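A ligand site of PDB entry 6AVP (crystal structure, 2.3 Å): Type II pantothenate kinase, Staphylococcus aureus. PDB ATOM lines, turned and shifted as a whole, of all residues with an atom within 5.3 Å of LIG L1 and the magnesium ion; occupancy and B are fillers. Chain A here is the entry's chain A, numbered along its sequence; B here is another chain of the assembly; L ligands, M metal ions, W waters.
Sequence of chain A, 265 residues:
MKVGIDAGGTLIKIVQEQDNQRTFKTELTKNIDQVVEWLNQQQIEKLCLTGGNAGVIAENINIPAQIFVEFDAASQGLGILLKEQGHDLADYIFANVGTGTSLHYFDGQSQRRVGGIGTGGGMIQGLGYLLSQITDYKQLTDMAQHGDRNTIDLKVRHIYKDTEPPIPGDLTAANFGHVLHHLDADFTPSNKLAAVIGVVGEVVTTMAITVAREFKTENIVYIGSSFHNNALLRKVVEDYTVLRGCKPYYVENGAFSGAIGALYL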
ATOM      1  N   ASP A   6      34.186  -5.966 -28.799  1.00  0.00           N
ATOM      2  CA  ASP A   6      33.372  -6.568 -27.740  1.00  0.00           C
ATOM      3  C   ASP A   6      32.204  -7.246 -28.449  1.00  0.00           C
ATOM      4  O   ASP A   6      31.290  -6.571 -28.923  1.00  0.00           O
ATOM      5  CB  ASP A   6      32.889  -5.482 -26.782  1.00  0.00           C
ATOM      6  CG  ASP A   6      31.978  -6.009 -25.669  1.00  0.00           C
ATOM      7  OD1 ASP A   6      31.457  -7.141 -25.758  1.00  0.00           O
ATOM      8  OD2 ASP A   6      31.759  -5.275 -24.682  1.00  0.00           O
ATOM      9  N   GLY A   8      29.168  -9.109 -28.075  1.00  0.00           N
ATOM     10  CA  GLY A   8      28.174  -9.416 -27.062  1.00  0.00           C
ATOM     11  C   GLY A   8      27.076 -10.326 -27.555  1.00  0.00           C
ATOM     12  O   GLY A   8      27.147 -10.901 -28.652  1.00  0.00           O
ATOM     13  N   GLY A   9      26.068 -10.458 -26.699  1.00  0.00           N
ATOM     14  CA  GLY A   9      24.934 -11.331 -26.941  1.00  0.00           C
ATOM     15  C   GLY A   9      24.047 -10.865 -28.067  1.00  0.00           C
ATOM     16  O   GLY A   9      23.459 -11.688 -28.762  1.00  0.00           O
ATOM     17  N   THR A  10      23.981  -9.547 -28.250  1.00  0.00           N
ATOM     18  CA  THR A  10      23.117  -8.921 -29.256  1.00  0.00           C
ATOM     19  C   THR A  10      23.898  -8.084 -30.278  1.00  0.00           C
ATOM     20  O   THR A  10      23.656  -8.178 -31.485  1.00  0.00           O
ATOM     21  CB  THR A  10      22.012  -8.069 -28.594  1.00  0.00           C
ATOM     22  OG1 THR A  10      21.353  -8.848 -27.577  1.00  0.00           O
ATOM     23  CG2 THR A  10      20.980  -7.615 -29.631  1.00  0.00           C
ATOM     24  N   LEU A  11      24.817  -7.242 -29.801  1.00  0.00           N
ATOM     25  CA  LEU A  11      25.620  -6.372 -30.675  1.00  0.00           C
ATOM     26  C   LEU A  11      27.134  -6.672 -30.597  1.00  0.00           C
ATOM     27  O   LEU A  11      27.672  -7.075 -29.555  1.00  0.00           O
ATOM     28  CB  LEU A  11      25.361  -4.903 -30.337  1.00  0.00           C
ATOM     29  CG  LEU A  11      23.892  -4.468 -30.500  1.00  0.00           C
ATOM     30  CD1 LEU A  11      23.577  -3.154 -29.769  1.00  0.00           C
ATOM     31  CD2 LEU A  11      23.508  -4.379 -31.972  1.00  0.00           C
ATOM     32  N   ILE A  12      27.779  -6.495 -31.738  1.00  0.00           N
ATOM     33  CA  ILE A  12      29.230  -6.515 -31.828  1.00  0.00           C
ATOM     34  C   ILE A  12      29.675  -5.055 -31.909  1.00  0.00           C
ATOM     35  O   ILE A  12      29.202  -4.321 -32.804  1.00  0.00           O
ATOM     36  CB  ILE A  12      29.688  -7.277 -33.081  1.00  0.00           C
ATOM     37  CG1 ILE A  12      29.280  -8.744 -32.967  1.00  0.00           C
ATOM     38  CG2 ILE A  12      31.203  -7.150 -33.260  1.00  0.00           C
ATOM     39  CD1 ILE A  12      29.422  -9.529 -34.256  1.00  0.00           C
ATOM     40  N   LYS A  13      30.557  -4.641 -31.015  1.00  0.00           N
ATOM     41  CA  LYS A  13      31.084  -3.272 -31.012  1.00  0.00           C
ATOM     42  C   LYS A  13      32.525  -3.301 -31.420  1.00  0.00           C
ATOM     43  O   LYS A  13      33.317  -4.027 -30.862  1.00  0.00           O
ATOM     44  CB  LYS A  13      30.988  -2.596 -29.654  1.00  0.00           C
ATOM     45  CG  LYS A  13      29.577  -2.361 -29.168  1.00  0.00           C
ATOM     46  CD  LYS A  13      29.271  -3.294 -28.010  1.00  0.00           C
ATOM     47  CE  LYS A  13      28.071  -4.149 -28.265  1.00  0.00           C
ATOM     48  NZ  LYS A  13      28.011  -5.316 -27.338  1.00  0.00           N
ATOM     49  N   LEU A  28      25.215  -6.180 -35.791  1.00  0.00           N
ATOM     50  CA  LEU A  28      24.506  -7.244 -35.135  1.00  0.00           C
ATOM     51  C   LEU A  28      25.377  -8.501 -34.919  1.00  0.00           C
ATOM     52  O   LEU A  28      26.217  -8.848 -35.747  1.00  0.00           O
ATOM     53  CB  LEU A  28      23.253  -7.614 -35.903  1.00  0.00           C
ATOM     54  CG  LEU A  28      22.042  -6.737 -35.647  1.00  0.00           C
ATOM     55  CD1 LEU A  28      21.823  -5.790 -36.803  1.00  0.00           C
ATOM     56  CD2 LEU A  28      20.812  -7.627 -35.493  1.00  0.00           C
ATOM     57  N   THR A  29      25.138  -9.158 -33.792  1.00  0.00           N
ATOM     58  CA  THR A  29      25.784 -10.433 -33.455  1.00  0.00           C
ATOM     59  C   THR A  29      25.353 -11.568 -34.403  1.00  0.00           C
ATOM     60  O   THR A  29      26.125 -12.501 -34.671  1.00  0.00           O
ATOM     61  CB  THR A  29      25.494 -10.804 -31.993  1.00  0.00           C
ATOM     62  OG1 THR A  29      26.152  -9.868 -31.139  1.00  0.00           O
ATOM     63  CG2 THR A  29      25.988 -12.206 -31.667  1.00  0.00           C
ATOM     64  N   GLU A  70      35.452  -9.647 -20.303  1.00  0.00           N
ATOM     65  CA  GLU A  70      34.675  -8.414 -20.573  1.00  0.00           C
ATOM     66  C   GLU A  70      34.457  -7.479 -19.374  1.00  0.00           C
ATOM     67  O   GLU A  70      34.225  -6.272 -19.579  1.00  0.00           O
ATOM     68  CB  GLU A  70      33.307  -8.750 -21.206  1.00  0.00           C
ATOM     69  CG  GLU A  70      32.333  -9.561 -20.354  1.00  0.00           C
ATOM     70  CD  GLU A  70      30.915  -9.587 -20.920  1.00  0.00           C
ATOM     71  OE1 GLU A  70      30.136  -8.674 -20.592  1.00  0.00           O
ATOM     72  OE2 GLU A  70      30.565 -10.520 -21.679  1.00  0.00           O
ATOM     73  N   ASN A  96      26.529  -2.204 -16.247  1.00  0.00           N
ATOM     74  CA  ASN A  96      26.533  -2.490 -17.690  1.00  0.00           C
ATOM     75  C   ASN A  96      25.185  -3.106 -18.107  1.00  0.00           C
ATOM     76  O   ASN A  96      24.909  -4.293 -17.846  1.00  0.00           O
ATOM     77  CB  ASN A  96      27.657  -3.463 -17.957  1.00  0.00           C
ATOM     78  CG  ASN A  96      28.022  -3.558 -19.403  1.00  0.00           C
ATOM     79  OD1 ASN A  96      27.216  -3.272 -20.287  1.00  0.00           O
ATOM     80  ND2 ASN A  96      29.248  -3.929 -19.657  1.00  0.00           N
ATOM     81  N   VAL A  97      24.337  -2.280 -18.729  1.00  0.00           N
ATOM     82  CA  VAL A  97      22.975  -2.680 -19.073  1.00  0.00           C
ATOM     83  C   VAL A  97      22.969  -3.141 -20.535  1.00  0.00           C
ATOM     84  O   VAL A  97      22.711  -2.365 -21.445  1.00  0.00           O
ATOM     85  CB  VAL A  97      21.966  -1.534 -18.826  1.00  0.00           C
ATOM     86  CG1 VAL A  97      20.554  -2.017 -19.033  1.00  0.00           C
ATOM     87  CG2 VAL A  97      22.093  -1.009 -17.414  1.00  0.00           C
ATOM     88  N   GLY A  98      23.282  -4.413 -20.749  1.00  0.00           N
ATOM     89  CA  GLY A  98      23.379  -4.984 -22.105  1.00  0.00           C
ATOM     90  C   GLY A  98      22.212  -5.901 -22.380  1.00  0.00           C
ATOM     91  O   GLY A  98      21.105  -5.645 -21.898  1.00  0.00           O
ATOM     92  N   THR A  99      22.433  -6.958 -23.159  1.00  0.00           N
ATOM     93  CA  THR A  99      21.419  -7.992 -23.307  1.00  0.00           C
ATOM     94  C   THR A  99      20.936  -8.415 -21.911  1.00  0.00           C
ATOM     95  O   THR A  99      19.743  -8.608 -21.713  1.00  0.00           O
ATOM     96  CB  THR A  99      21.967  -9.227 -24.039  1.00  0.00           C
ATOM     97  OG1 THR A  99      22.561  -8.830 -25.278  1.00  0.00           O
ATOM     98  CG2 THR A  99      20.864 -10.223 -24.310  1.00  0.00           C
ATOM     99  N   GLY A 100      21.901  -8.606 -21.004  1.00  0.00           N
ATOM    100  CA  GLY A 100      21.682  -8.789 -19.575  1.00  0.00           C
ATOM    101  C   GLY A 100      22.394  -7.678 -18.802  1.00  0.00           C
ATOM    102  O   GLY A 100      22.955  -6.785 -19.388  1.00  0.00           O
ATOM    103  N   GLY A 121      18.406  -5.071 -21.692  1.00  0.00           N
ATOM    104  CA  GLY A 121      17.997  -4.878 -23.087  1.00  0.00           C
ATOM    105  C   GLY A 121      17.325  -6.070 -23.744  1.00  0.00           C
ATOM    106  O   GLY A 121      16.431  -5.911 -24.600  1.00  0.00           O
ATOM    107  N   GLY A 122      17.735  -7.266 -23.354  1.00  0.00           N
ATOM    108  CA  GLY A 122      17.161  -8.493 -23.886  1.00  0.00           C
ATOM    109  C   GLY A 122      15.727  -8.688 -23.420  1.00  0.00           C
ATOM    110  O   GLY A 122      14.877  -9.191 -24.155  1.00  0.00           O
ATOM    111  N   ILE A 124      13.809  -6.099 -22.605  1.00  0.00           N
ATOM    112  CA  ILE A 124      13.101  -5.026 -23.315  1.00  0.00           C
ATOM    113  C   ILE A 124      12.663  -5.538 -24.685  1.00  0.00           C
ATOM    114  O   ILE A 124      11.500  -5.445 -25.021  1.00  0.00           O
ATOM    115  CB  ILE A 124      13.937  -3.719 -23.379  1.00  0.00           C
ATOM    116  CG1 ILE A 124      14.095  -3.156 -21.964  1.00  0.00           C
ATOM    117  CG2 ILE A 124      13.222  -2.677 -24.250  1.00  0.00           C
ATOM    118  CD1 ILE A 124      14.983  -1.939 -21.819  1.00  0.00           C
ATOM    119  N   GLN A 125      13.592  -6.109 -25.441  1.00  0.00           N
ATOM    120  CA  GLN A 125      13.258  -6.702 -26.744  1.00  0.00           C
ATOM    121  C   GLN A 125      12.339  -7.908 -26.670  1.00  0.00           C
ATOM    122  O   GLN A 125      11.360  -7.986 -27.416  1.00  0.00           O
ATOM    123  CB  GLN A 125      14.517  -7.077 -27.511  1.00  0.00           C
ATOM    124  CG  GLN A 125      15.287  -5.879 -28.043  1.00  0.00           C
ATOM    125  CD  GLN A 125      16.384  -6.289 -28.988  1.00  0.00           C
ATOM    126  OE1 GLN A 125      16.320  -6.018 -30.170  1.00  0.00           O
ATOM    127  NE2 GLN A 125      17.413  -6.963 -28.462  1.00  0.00           N
ATOM    128  N   TYR A 137      13.881  -2.972 -33.356  1.00  0.00           N
ATOM    129  CA  TYR A 137      14.311  -2.276 -32.135  1.00  0.00           C
ATOM    130  C   TYR A 137      13.921  -0.795 -32.128  1.00  0.00           C
ATOM    131  O   TYR A 137      13.469  -0.244 -31.105  1.00  0.00           O
ATOM    132  CB  TYR A 137      15.831  -2.426 -31.898  1.00  0.00           C
ATOM    133  CG  TYR A 137      16.327  -1.643 -30.700  1.00  0.00           C
ATOM    134  CD1 TYR A 137      16.144  -2.102 -29.412  1.00  0.00           C
ATOM    135  CD2 TYR A 137      16.957  -0.403 -30.853  1.00  0.00           C
ATOM    136  CE1 TYR A 137      16.574  -1.383 -28.313  1.00  0.00           C
ATOM    137  CE2 TYR A 137      17.384   0.330 -29.756  1.00  0.00           C
ATOM    138  CZ  TYR A 137      17.201  -0.161 -28.479  1.00  0.00           C
ATOM    139  OH  TYR A 137      17.634   0.539 -27.369  1.00  0.00           O
ATOM    140  N   GLY A 224      26.170   0.534 -21.605  1.00  0.00           N
ATOM    141  CA  GLY A 224      25.489  -0.485 -22.396  1.00  0.00           C
ATOM    142  C   GLY A 224      24.698   0.142 -23.538  1.00  0.00           C
ATOM    143  O   GLY A 224      24.339   1.316 -23.471  1.00  0.00           O
ATOM    144  N   SER A 225      24.438  -0.616 -24.589  1.00  0.00           N
ATOM    145  CA  SER A 225      23.661  -0.124 -25.718  1.00  0.00           C
ATOM    146  C   SER A 225      22.165  -0.003 -25.417  1.00  0.00           C
ATOM    147  O   SER A 225      21.474   0.638 -26.174  1.00  0.00           O
ATOM    148  CB  SER A 225      23.851  -1.006 -26.954  1.00  0.00           C
ATOM    149  OG  SER A 225      25.195  -1.376 -27.118  1.00  0.00           O
ATOM    150  N   SER A 226      21.673  -0.627 -24.345  1.00  0.00           N
ATOM    151  CA  SER A 226      20.251  -0.538 -23.954  1.00  0.00           C
ATOM    152  C   SER A 226      19.721   0.873 -23.900  1.00  0.00           C
ATOM    153  O   SER A 226      18.527   1.093 -24.069  1.00  0.00           O
ATOM    154  CB  SER A 226      20.014  -1.178 -22.578  1.00  0.00           C
ATOM    155  OG  SER A 226      20.110  -2.581 -22.657  1.00  0.00           O
ATOM    156  N   HIS A 228      20.639   3.359 -25.990  1.00  0.00           N
ATOM    157  CA  HIS A 228      20.564   3.983 -27.283  1.00  0.00           C
ATOM    158  C   HIS A 228      19.107   4.049 -27.744  1.00  0.00           C
ATOM    159  O   HIS A 228      18.397   3.047 -27.677  1.00  0.00           O
ATOM    160  CB  HIS A 228      21.402   3.255 -28.331  1.00  0.00           C
ATOM    161  CG  HIS A 228      21.259   3.841 -29.704  1.00  0.00           C
ATOM    162  ND1 HIS A 228      20.399   3.313 -30.644  1.00  0.00           N
ATOM    163  CD2 HIS A 228      21.810   4.936 -30.265  1.00  0.00           C
ATOM    164  CE1 HIS A 228      20.450   4.054 -31.750  1.00  0.00           C
ATOM    165  NE2 HIS A 228      21.305   5.038 -31.542  1.00  0.00           N
ATOM    166  N   ALA A 255      28.688   2.486 -24.360  1.00  0.00           N
ATOM    167  CA  ALA A 255      28.447   1.134 -24.894  1.00  0.00           C
ATOM    168  C   ALA A 255      29.664   0.491 -25.610  1.00  0.00           C
ATOM    169  O   ALA A 255      29.610  -0.687 -25.961  1.00  0.00           O
ATOM    170  CB  ALA A 255      27.247   1.166 -25.836  1.00  0.00           C
ATOM    171  N   ILE B 159      25.014 -16.858 -24.463  1.00  0.00           N
ATOM    172  CA  ILE B 159      25.817 -15.708 -24.891  1.00  0.00           C
ATOM    173  C   ILE B 159      27.262 -16.148 -25.131  1.00  0.00           C
ATOM    174  O   ILE B 159      27.892 -15.708 -26.065  1.00  0.00           O
ATOM    175  CB  ILE B 159      25.765 -14.549 -23.860  1.00  0.00           C
ATOM    176  CG1 ILE B 159      24.394 -13.871 -23.916  1.00  0.00           C
ATOM    177  CG2 ILE B 159      26.847 -13.506 -24.115  1.00  0.00           C
ATOM    178  CD1 ILE B 159      24.147 -12.859 -22.822  1.00  0.00           C
HETATM  179  P1  LIG L   1      25.690  -7.013 -25.585  1.00  0.00           P
HETATM  180  O1  LIG L   1      25.115  -8.277 -24.987  1.00  0.00           O
HETATM  181  O2  LIG L   1      27.070  -6.659 -25.076  1.00  0.00           O
HETATM  182  O3  LIG L   1      25.568  -6.961 -27.079  1.00  0.00           O
HETATM  183  P2  LIG L   1      24.711  -4.314 -25.531  1.00  0.00           P
HETATM  184  O4  LIG L   1      24.965  -3.343 -24.397  1.00  0.00           O
HETATM  185  O5  LIG L   1      25.542  -4.198 -26.763  1.00  0.00           O
HETATM  186  O6  LIG L   1      24.707  -5.845 -25.010  1.00  0.00           O
HETATM  187  O7  LIG L   1      23.209  -3.978 -25.992  1.00  0.00           O
HETATM  188  C1  LIG L   1      22.135  -4.872 -26.187  1.00  0.00           C
HETATM  189  C2  LIG L   1      20.835  -4.090 -26.127  1.00  0.00           C
HETATM  190  O8  LIG L   1      20.884  -2.787 -26.704  1.00  0.00           O
HETATM  191  C3  LIG L   1      19.712  -4.804 -26.849  1.00  0.00           C
HETATM  192  O9  LIG L   1      19.259  -5.906 -26.055  1.00  0.00           O
HETATM  193  C4  LIG L   1      18.706  -3.681 -27.054  1.00  0.00           C
HETATM  194  O10 LIG L   1      17.879  -3.449 -25.900  1.00  0.00           O
HETATM  195  C5  LIG L   1      19.594  -2.447 -27.258  1.00  0.00           C
HETATM  196  N1  LIG L   1      19.825  -2.021 -28.669  1.00  0.00           N
HETATM  197  C6  LIG L   1      20.333  -0.819 -28.989  1.00  0.00           C
HETATM  198  N2  LIG L   1      20.471  -0.689 -30.322  1.00  0.00           N
HETATM  199  C7  LIG L   1      20.083  -1.839 -30.881  1.00  0.00           C
HETATM  200  C8  LIG L   1      19.994  -2.371 -32.261  1.00  0.00           C
HETATM  201  N3  LIG L   1      20.364  -1.620 -33.328  1.00  0.00           N
HETATM  202  N4  LIG L   1      19.524  -3.629 -32.416  1.00  0.00           N
HETATM  203  C9  LIG L   1      19.162  -4.390 -31.368  1.00  0.00           C
HETATM  204  N5  LIG L   1      19.230  -3.950 -30.108  1.00  0.00           N
HETATM  205  C10 LIG L   1      19.661  -2.718 -29.797  1.00  0.00           C
HETATM  206  O1  LG2 L   2      24.856  -8.714 -21.420  1.00  0.00           O
HETATM  207  P1  LG2 L   2      26.199  -8.878 -22.117  1.00  0.00           P
HETATM  208  O2  LG2 L   2      27.088  -7.717 -22.237  1.00  0.00           O
HETATM  209  O3  LG2 L   2      26.335  -9.915 -23.156  1.00  0.00           O
HETATM  210  O4  LG2 L   2      27.031  -9.624 -20.913  1.00  0.00           O
HETATM  211  C1  LG2 L   2      26.745 -11.002 -20.557  1.00  0.00           C
HETATM  212  C2  LG2 L   2      26.518 -11.199 -19.026  1.00  0.00           C
HETATM  213  C3  LG2 L   2      27.828 -10.870 -18.275  1.00  0.00           C
HETATM  214  C4  LG2 L   2      26.107 -12.662 -18.810  1.00  0.00           C
HETATM  215  C5  LG2 L   2      25.395 -10.245 -18.550  1.00  0.00           C
HETATM  216  O5  LG2 L   2      24.277 -10.390 -19.398  1.00  0.00           O
HETATM  217  C6  LG2 L   2      24.974 -10.524 -17.096  1.00  0.00           C
HETATM  218  O6  LG2 L   2      25.737 -10.336 -16.147  1.00  0.00           O
HETATM  219  N1  LG2 L   2      23.761 -11.083 -17.007  1.00  0.00           N
HETATM  220  C7  LG2 L   2      23.103 -11.418 -15.748  1.00  0.00           C
HETATM  221  C8  LG2 L   2      23.670 -12.688 -15.161  1.00  0.00           C
HETATM  222  C9  LG2 L   2      23.255 -12.703 -13.686  1.00  0.00           C
HETATM  223  O7  LG2 L   2      23.940 -12.099 -12.866  1.00  0.00           O
HETATM  224  N2  LG2 L   2      22.113 -13.351 -13.376  1.00  0.00           N
HETATM  225  C10 LG2 L   2      21.739 -13.483 -11.987  1.00  0.00           C
HETATM  226  C11 LG2 L   2      20.249 -13.510 -11.857  1.00  0.00           C
HETATM  227  C12 LG2 L   2      19.860 -14.842 -11.195  1.00  0.00           C
HETATM  228  C13 LG2 L   2      19.915 -15.917 -12.251  1.00  0.00           C
HETATM  229  C14 LG2 L   2      19.299 -17.172 -11.673  1.00  0.00           C
HETATM  230  O8  LG2 L   2      19.608 -18.211 -12.674  1.00  0.00           O
HETATM  231  C15 LG2 L   2      18.895 -19.438 -12.500  1.00  0.00           C
HETATM  232 MG    MG M   1      28.193  -6.347 -23.519  1.00  0.00          MG
HETATM  233  O   HOH W   1      29.086  -5.929 -21.365  1.00  0.00           O
HETATM  234  O   HOH W   2      29.720  -7.619 -23.689  1.00  0.00           O
HETATM  235  O   HOH W   3      29.117  -4.942 -24.616  1.00  0.00           O
HETATM  236  O   HOH W   4      26.866  -4.886 -22.546  1.00  0.00           O
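The side-chain amino group (NZ) of Lys 13 sits at hydrogen-bond distance from the backbone carbonyl oxygen (O) of Leu 11.
The backbone NH (N) of Gly 121 is in hydrogen-bond range of the backbone carbonyl oxygen (O) of Gly 98.
The side-chain hydroxyl (OG) of Ser 226 lies close to the backbone NH (N) of Gly 121, at 3.2 Å.
The side-chain hydroxyl (OH) of Tyr 137 is in hydrogen-bond range of the backbone carbonyl oxygen (O) of Ser 226 (3.5 Å).
O of Gly 98 sits at hydrogen-bond distance from OG of Ser 226 (3.3 Å).
The backbone carbonyl oxygen of Thr 10 sits at hydrogen-bond distance from the backbone NH of Thr 29 (2.9 Å).
The backbone carbonyl oxygen of Val 97 is in hydrogen-bond range of the side-chain hydroxyl of Ser 226, 2.9 Å away.
The side-chain hydroxyl of Thr 29 sits at hydrogen-bond distance from the backbone carbonyl oxygen of Gly 8, 2.9 Å away.
The magnesium ion is bound by an oxygen (O2) of LIG L1 (1.9 Å), water W2 (2.0 Å), water W3 (2.0 Å), an oxygen (O2) of LG2 L2 (2.2 Å), water W4 (2.2 Å) and water W1 (2.4 Å).
Merely in contact with the magnesium ion: Asp 6 and Lys 13.
Of the 26 residues printed, 2 come within 4 Å of the magnesium ion.
The nearest printed residue that does not touch the magnesium ion is Glu 70 (4.2 Å).
CA of Gly 8 touches O2 of LIG L1 (3.6 Å).
Val 97 touches LIG L1.
CA of Gly 98 touches O4 of LIG L1, at 3.2 Å.
CZ of Tyr 137 touches N1 of LIG L1, 3.2 Å away.
Gly 224 touches LIG L1.
Hydrophobic or aromatic side chains that line LIG L1: Leu 11 and Tyr 137.
Within 4 Å of LIG L1: Gly 8, Gly 9, Thr 10, Leu 11, Lys 13, Val 97, Gly 98, Thr 99, Gly 121, Gly 122, Gln 125, Tyr 137, Gly 224, Ser 225 and Ser 226.
The nearest printed residue that does not touch LIG L1 is His 228 (4.02 Å).
O6 of LIG L1 is in hydrogen-bond range of N of Thr 99, 3.1 Å away.
The side-chain hydroxyl (OG1) of Thr 99 lies within hydrogen-bond range of an oxygen (O1) of LIG L1 (2.6 Å).
An oxygen (O5) of LIG L1 is in salt-bridge range of the side-chain amino group of Lys 13 (2.8 Å).
The backbone NH (N) of Ser 225 sits at hydrogen-bond distance from an oxygen (O4) of LIG L1 (2.8 Å).
The side-chain hydroxyl of Ser 225 is in hydrogen-bond range of an oxygen (O5) of LIG L1, at 2.9 Å.
N of Leu 11 is in hydrogen-bond range of O3 of LIG L1, at 2.8 Å.
The backbone NH of Gly 9 lies within hydrogen-bond range of an oxygen (O1) of LIG L1, at 2.9 Å.
An oxygen (O10) of LIG L1 is in hydrogen-bond range of the backbone carbonyl oxygen (O) of Gly 121, at 3.1 Å.
The side-chain amide nitrogen (NE2) of Gln 125 sits at hydrogen-bond distance from an oxygen (O9) of LIG L1.
O3 of LIG L1 lies within hydrogen-bond range of N of Thr 10, 3.3 Å away.
The backbone NH (N) of Ser 226 is in hydrogen-bond range of an oxygen (O8) of LIG L1.
N of Gly 122 is in hydrogen-bond range of O9 of LIG L1 (3.4 Å).
An oxygen (O1) of LG2 L2 lies within hydrogen-bond range of the backbone NH (N) of Thr 99 (3.5 Å).
O1 of LG2 L2 sits at hydrogen-bond distance from N of Gly 100 (3.0 Å).
Water W1 bridges ND2 of Asn 96 and OE1 of Glu 70.
Water W3 bridges the side-chain carboxylate (OD2) of Asp 6 (2.7 Å) and the side-chain amino group (NZ) of Lys 13 (3.0 Å).
Water W4 bridges the side-chain amide oxygen (OD1) of Asn 96 (2.8 Å) and an oxygen (O4) of LIG L1 (3.1 Å).
Water W2 lies within hydrogen-bond range of OD1 of Asp 6 (2.7 Å) and OE1 of Glu 70 (3.3 Å).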
